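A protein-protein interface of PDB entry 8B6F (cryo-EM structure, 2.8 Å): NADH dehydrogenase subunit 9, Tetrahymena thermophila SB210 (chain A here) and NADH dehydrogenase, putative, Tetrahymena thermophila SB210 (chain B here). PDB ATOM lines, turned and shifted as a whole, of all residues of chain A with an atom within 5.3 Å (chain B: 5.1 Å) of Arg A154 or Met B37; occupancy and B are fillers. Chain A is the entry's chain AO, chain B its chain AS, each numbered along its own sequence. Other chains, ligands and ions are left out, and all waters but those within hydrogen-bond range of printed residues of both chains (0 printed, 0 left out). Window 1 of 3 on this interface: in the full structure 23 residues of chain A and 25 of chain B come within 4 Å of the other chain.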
ATOM      1  N   ARG A 137      29.529 -14.654 -17.580  1.00  0.00           N
ATOM      2  CA  ARG A 137      28.490 -13.663 -17.837  1.00  0.00           C
ATOM      3  C   ARG A 137      29.020 -12.561 -18.742  1.00  0.00           C
ATOM      4  O   ARG A 137      28.358 -12.161 -19.706  1.00  0.00           O
ATOM      5  CB  ARG A 137      27.975 -13.076 -16.521  1.00  0.00           C
ATOM      6  CG  ARG A 137      27.169 -14.057 -15.684  1.00  0.00           C
ATOM      7  CD  ARG A 137      26.814 -13.480 -14.325  1.00  0.00           C
ATOM      8  NE  ARG A 137      25.964 -12.303 -14.432  1.00  0.00           N
ATOM      9  CZ  ARG A 137      25.502 -11.617 -13.396  1.00  0.00           C
ATOM     10  NH1 ARG A 137      25.789 -11.964 -12.153  1.00  0.00           N
ATOM     11  NH2 ARG A 137      24.729 -10.557 -13.612  1.00  0.00           N
ATOM     12  N   ASP A 152      24.093 -18.275 -13.363  1.00  0.00           N
ATOM     13  CA  ASP A 152      23.419 -16.991 -13.521  1.00  0.00           C
ATOM     14  C   ASP A 152      23.738 -16.435 -14.898  1.00  0.00           C
ATOM     15  O   ASP A 152      24.896 -16.123 -15.185  1.00  0.00           O
ATOM     16  CB  ASP A 152      23.857 -16.010 -12.427  1.00  0.00           C
ATOM     17  CG  ASP A 152      23.075 -14.713 -12.456  1.00  0.00           C
ATOM     18  OD1 ASP A 152      22.183 -14.570 -13.317  1.00  0.00           O
ATOM     19  OD2 ASP A 152      23.349 -13.838 -11.611  1.00  0.00           O
ATOM     20  N   THR A 153      22.718 -16.307 -15.741  1.00  0.00           N
ATOM     21  CA  THR A 153      22.886 -15.803 -17.097  1.00  0.00           C
ATOM     22  C   THR A 153      22.633 -14.306 -17.216  1.00  0.00           C
ATOM     23  O   THR A 153      22.762 -13.759 -18.315  1.00  0.00           O
ATOM     24  CB  THR A 153      21.951 -16.545 -18.055  1.00  0.00           C
ATOM     25  OG1 THR A 153      20.592 -16.365 -17.639  1.00  0.00           O
ATOM     26  CG2 THR A 153      22.279 -18.023 -18.079  1.00  0.00           C
ATOM     27  N   ARG A 154      22.284 -13.632 -16.126  1.00  0.00           N
ATOM     28  CA  ARG A 154      21.970 -12.213 -16.194  1.00  0.00           C
ATOM     29  C   ARG A 154      23.204 -11.407 -16.589  1.00  0.00           C
ATOM     30  O   ARG A 154      24.339 -11.772 -16.279  1.00  0.00           O
ATOM     31  CB  ARG A 154      21.417 -11.732 -14.853  1.00  0.00           C
ATOM     32  CG  ARG A 154      19.978 -12.168 -14.613  1.00  0.00           C
ATOM     33  CD  ARG A 154      19.572 -12.082 -13.149  1.00  0.00           C
ATOM     34  NE  ARG A 154      20.011 -10.844 -12.518  1.00  0.00           N
ATOM     35  CZ  ARG A 154      21.051 -10.733 -11.703  1.00  0.00           C
ATOM     36  NH1 ARG A 154      21.789 -11.781 -11.371  1.00  0.00           N
ATOM     37  NH2 ARG A 154      21.363  -9.539 -11.209  1.00  0.00           N
ATOM     38  N   LYS A 155      22.967 -10.301 -17.289  1.00  0.00           N
ATOM     39  CA  LYS A 155      24.055  -9.498 -17.825  1.00  0.00           C
ATOM     40  C   LYS A 155      24.880  -8.877 -16.703  1.00  0.00           C
ATOM     41  O   LYS A 155      24.411  -8.671 -15.581  1.00  0.00           O
ATOM     42  CB  LYS A 155      23.519  -8.391 -18.733  1.00  0.00           C
ATOM     43  CG  LYS A 155      22.866  -8.893 -20.010  1.00  0.00           C
ATOM     44  CD  LYS A 155      22.429  -7.744 -20.908  1.00  0.00           C
ATOM     45  CE  LYS A 155      21.335  -6.902 -20.264  1.00  0.00           C
ATOM     46  NZ  LYS A 155      20.858  -5.820 -21.172  1.00  0.00           N
ATOM     47  N   LEU A 156      26.132  -8.575 -17.032  1.00  0.00           N
ATOM     48  CA  LEU A 156      27.066  -7.969 -16.091  1.00  0.00           C
ATOM     49  C   LEU A 156      27.984  -7.051 -16.881  1.00  0.00           C
ATOM     50  O   LEU A 156      28.759  -7.532 -17.709  1.00  0.00           O
ATOM     51  CB  LEU A 156      27.874  -9.042 -15.357  1.00  0.00           C
ATOM     52  CG  LEU A 156      28.772  -8.575 -14.214  1.00  0.00           C
ATOM     53  CD1 LEU A 156      27.942  -8.244 -12.984  1.00  0.00           C
ATOM     54  CD2 LEU A 156      29.812  -9.628 -13.895  1.00  0.00           C
ATOM     55  N   TYR B   4      13.716 -17.607  -7.469  1.00  0.00           N
ATOM     56  CA  TYR B   4      12.985 -16.349  -7.358  1.00  0.00           C
ATOM     57  C   TYR B   4      11.497 -16.540  -7.623  1.00  0.00           C
ATOM     58  O   TYR B   4      10.669 -15.816  -7.061  1.00  0.00           O
ATOM     59  CB  TYR B   4      13.565 -15.315  -8.320  1.00  0.00           C
ATOM     60  CG  TYR B   4      12.835 -13.996  -8.281  1.00  0.00           C
ATOM     61  CD1 TYR B   4      12.990 -13.128  -7.210  1.00  0.00           C
ATOM     62  CD2 TYR B   4      11.994 -13.618  -9.315  1.00  0.00           C
ATOM     63  CE1 TYR B   4      12.323 -11.920  -7.170  1.00  0.00           C
ATOM     64  CE2 TYR B   4      11.323 -12.413  -9.285  1.00  0.00           C
ATOM     65  CZ  TYR B   4      11.493 -11.569  -8.209  1.00  0.00           C
ATOM     66  OH  TYR B   4      10.826 -10.369  -8.175  1.00  0.00           O
ATOM     67  N   TRP B   5      11.141 -17.500  -8.470  1.00  0.00           N
ATOM     68  CA  TRP B   5       9.755 -17.791  -8.803  1.00  0.00           C
ATOM     69  C   TRP B   5       9.145 -18.858  -7.905  1.00  0.00           C
ATOM     70  O   TRP B   5       8.007 -19.273  -8.143  1.00  0.00           O
ATOM     71  CB  TRP B   5       9.653 -18.230 -10.263  1.00  0.00           C
ATOM     72  CG  TRP B   5       9.993 -17.151 -11.241  1.00  0.00           C
ATOM     73  CD1 TRP B   5       9.772 -15.813 -11.095  1.00  0.00           C
ATOM     74  CD2 TRP B   5      10.621 -17.317 -12.515  1.00  0.00           C
ATOM     75  NE1 TRP B   5      10.220 -15.137 -12.201  1.00  0.00           N
ATOM     76  CE2 TRP B   5      10.744 -16.038 -13.090  1.00  0.00           C
ATOM     77  CE3 TRP B   5      11.086 -18.426 -13.229  1.00  0.00           C
ATOM     78  CZ2 TRP B   5      11.317 -15.836 -14.341  1.00  0.00           C
ATOM     79  CZ3 TRP B   5      11.654 -18.224 -14.473  1.00  0.00           C
ATOM     80  CH2 TRP B   5      11.764 -16.938 -15.017  1.00  0.00           C
ATOM     81  N   GLU B  35      12.126 -12.049  -1.832  1.00  0.00           N
ATOM     82  CA  GLU B  35      13.579 -12.024  -1.895  1.00  0.00           C
ATOM     83  C   GLU B  35      14.041 -11.684  -3.307  1.00  0.00           C
ATOM     84  O   GLU B  35      13.396 -12.042  -4.296  1.00  0.00           O
ATOM     85  CB  GLU B  35      14.162 -13.373  -1.471  1.00  0.00           C
ATOM     86  CG  GLU B  35      13.653 -13.872  -0.129  1.00  0.00           C
ATOM     87  CD  GLU B  35      14.353 -15.140   0.324  1.00  0.00           C
ATOM     88  OE1 GLU B  35      15.595 -15.201   0.225  1.00  0.00           O
ATOM     89  OE2 GLU B  35      13.661 -16.079   0.771  1.00  0.00           O
ATOM     90  N   ILE B  36      15.175 -10.990  -3.393  1.00  0.00           N
ATOM     91  CA  ILE B  36      15.722 -10.575  -4.681  1.00  0.00           C
ATOM     92  C   ILE B  36      16.252 -11.796  -5.419  1.00  0.00           C
ATOM     93  O   ILE B  36      16.431 -12.865  -4.827  1.00  0.00           O
ATOM     94  CB  ILE B  36      16.825  -9.514  -4.512  1.00  0.00           C
ATOM     95  CG1 ILE B  36      17.998 -10.078  -3.703  1.00  0.00           C
ATOM     96  CG2 ILE B  36      16.248  -8.270  -3.849  1.00  0.00           C
ATOM     97  CD1 ILE B  36      19.174  -9.131  -3.574  1.00  0.00           C
ATOM     98  N   MET B  37      16.507 -11.643  -6.716  1.00  0.00           N
ATOM     99  CA  MET B  37      17.000 -12.730  -7.556  1.00  0.00           C
ATOM    100  C   MET B  37      18.522 -12.751  -7.481  1.00  0.00           C
ATOM    101  O   MET B  37      19.192 -11.877  -8.038  1.00  0.00           O
ATOM    102  CB  MET B  37      16.520 -12.549  -8.994  1.00  0.00           C
ATOM    103  CG  MET B  37      16.980 -13.640  -9.947  1.00  0.00           C
ATOM    104  SD  MET B  37      16.450 -13.337 -11.642  1.00  0.00           S
ATOM    105  CE  MET B  37      14.682 -13.575 -11.499  1.00  0.00           C
ATOM    106  N   GLU B  38      19.069 -13.752  -6.790  1.00  0.00           N
ATOM    107  CA  GLU B  38      20.515 -13.885  -6.659  1.00  0.00           C
ATOM    108  C   GLU B  38      21.134 -14.659  -7.811  1.00  0.00           C
ATOM    109  O   GLU B  38      22.317 -14.467  -8.110  1.00  0.00           O
ATOM    110  CB  GLU B  38      20.859 -14.573  -5.334  1.00  0.00           C
ATOM    111  CG  GLU B  38      22.272 -14.311  -4.832  1.00  0.00           C
ATOM    112  CD  GLU B  38      23.323 -15.168  -5.518  1.00  0.00           C
ATOM    113  OE1 GLU B  38      22.955 -16.193  -6.130  1.00  0.00           O
ATOM    114  OE2 GLU B  38      24.518 -14.814  -5.440  1.00  0.00           O
ATOM    115  N   ARG B  39      20.367 -15.529  -8.462  1.00  0.00           N
ATOM    116  CA  ARG B  39      20.880 -16.327  -9.564  1.00  0.00           C
ATOM    117  C   ARG B  39      19.719 -16.715 -10.465  1.00  0.00           C
ATOM    118  O   ARG B  39      18.635 -17.047  -9.981  1.00  0.00           O
ATOM    119  CB  ARG B  39      21.609 -17.577  -9.056  1.00  0.00           C
ATOM    120  CG  ARG B  39      20.767 -18.452  -8.140  1.00  0.00           C
ATOM    121  CD  ARG B  39      21.630 -19.357  -7.272  1.00  0.00           C
ATOM    122  NE  ARG B  39      22.244 -20.442  -8.028  1.00  0.00           N
ATOM    123  CZ  ARG B  39      23.124 -21.298  -7.526  1.00  0.00           C
ATOM    124  NH1 ARG B  39      23.534 -21.213  -6.272  1.00  0.00           N
ATOM    125  NH2 ARG B  39      23.602 -22.266  -8.301  1.00  0.00           N
ATOM    126  N   LEU B  40      19.954 -16.660 -11.776  1.00  0.00           N
ATOM    127  CA  LEU B  40      18.963 -17.033 -12.784  1.00  0.00           C
ATOM    128  C   LEU B  40      19.575 -18.120 -13.654  1.00  0.00           C
ATOM    129  O   LEU B  40      20.229 -17.820 -14.667  1.00  0.00           O
ATOM    130  CB  LEU B  40      18.549 -15.825 -13.620  1.00  0.00           C
ATOM    131  CG  LEU B  40      17.478 -16.073 -14.683  1.00  0.00           C
ATOM    132  CD1 LEU B  40      16.188 -16.579 -14.058  1.00  0.00           C
ATOM    133  CD2 LEU B  40      17.224 -14.810 -15.487  1.00  0.00           C
ATOM    134  N   GLU B 114      15.375 -11.651 -18.131  1.00  0.00           N
ATOM    135  CA  GLU B 114      16.213 -10.690 -17.425  1.00  0.00           C
ATOM    136  C   GLU B 114      15.631  -9.285 -17.513  1.00  0.00           C
ATOM    137  O   GLU B 114      15.542  -8.574 -16.507  1.00  0.00           O
ATOM    138  CB  GLU B 114      17.626 -10.721 -18.003  1.00  0.00           C
ATOM    139  CG  GLU B 114      18.554  -9.676 -17.421  1.00  0.00           C
ATOM    140  CD  GLU B 114      19.880  -9.637 -18.136  1.00  0.00           C
ATOM    141  OE1 GLU B 114      20.118 -10.513 -18.992  1.00  0.00           O
ATOM    142  OE2 GLU B 114      20.684  -8.731 -17.843  1.00  0.00           O
ATOM    143  N   TYR B 117      12.561  -8.937 -15.380  1.00  0.00           N
ATOM    144  CA  TYR B 117      12.916  -8.784 -13.973  1.00  0.00           C
ATOM    145  C   TYR B 117      13.398  -7.370 -13.681  1.00  0.00           C
ATOM    146  O   TYR B 117      13.061  -6.791 -12.642  1.00  0.00           O
ATOM    147  CB  TYR B 117      13.985  -9.803 -13.589  1.00  0.00           C
ATOM    148  CG  TYR B 117      14.480  -9.658 -12.171  1.00  0.00           C
ATOM    149  CD1 TYR B 117      13.778 -10.213 -11.111  1.00  0.00           C
ATOM    150  CD2 TYR B 117      15.653  -8.972 -11.893  1.00  0.00           C
ATOM    151  CE1 TYR B 117      14.228 -10.085  -9.815  1.00  0.00           C
ATOM    152  CE2 TYR B 117      16.111  -8.840 -10.598  1.00  0.00           C
ATOM    153  CZ  TYR B 117      15.394  -9.400  -9.565  1.00  0.00           C
ATOM    154  OH  TYR B 117      15.846  -9.270  -8.274  1.00  0.00           O
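The guanidinium group of Arg A137 is in salt-bridge range of the side-chain carboxylate of Asp A152 (3.1 Å).
NE of Arg A137 is in hydrogen-bond range of O of Arg A154 (2.5 Å).
NH2 of Arg A137 sits at hydrogen-bond distance from O of Lys A155 (2.7 Å).
The guanidinium group of Arg A154 is in salt-bridge range of the side-chain carboxylate of Asp A152 (2.6 Å).
The side-chain hydroxyl (OH) of Tyr B117 sits at hydrogen-bond distance from the backbone NH (N) of Met B37 (2.9 Å).
Of the printed residues of chain B, Arg A154 touches Met B37, Leu B40 and Glu B114.
Of the printed residues of chain A, Met B37 touches Arg A154 (3.7 Å).
Of the printed residues of chain A, Glu B38 touches Asp A152.
Of the printed residues of chain A, Arg B39 touches Asp A152 (3.97 Å).
The nearest residue of chain B that does not touch Arg A154 is Glu B38 (4.3 Å).
OD2 of Asp A152 touches O of Glu B38, 3.7 Å away.
CG of Asp A152 touches CA of Arg B39, at 3.97 Å.
Met B37 touches Arg A154 (SD to CD, 3.7 Å).
Leu B40 touches Arg A154 (CB to CD, 3.9 Å).
Arg A154 touches Glu B114 (CA to OE1, 3.8 Å).
Of the 6 printed residues of chain A, 4 touch a printed residue of chain B.
Of the 10 printed residues of chain B, 5 touch a printed residue of chain A.
Printed residues of chain B that touch a printed residue of chain A: Met B37, Glu B38, Arg B39, Leu B40 and Glu B114.
Hydrophobic or aromatic side chains of chain B within 4 Å of the printed part of chain A: Met B37 and Leu B40.
Among the printed residues, no Asp or Glu carboxylate lies within 4 Å of a Lys or Arg side-chain nitrogen of the other chain.
The backbone NH (N) of Leu B40 sits at hydrogen-bond distance from the side-chain carboxylate (OD1) of Asp A152 (3.4 Å).
N of Thr A153 is in hydrogen-bond range of O of Leu B40 (3.1 Å).
N of Lys A155 lies within hydrogen-bond range of OE2 of Glu B114 (2.8 Å).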
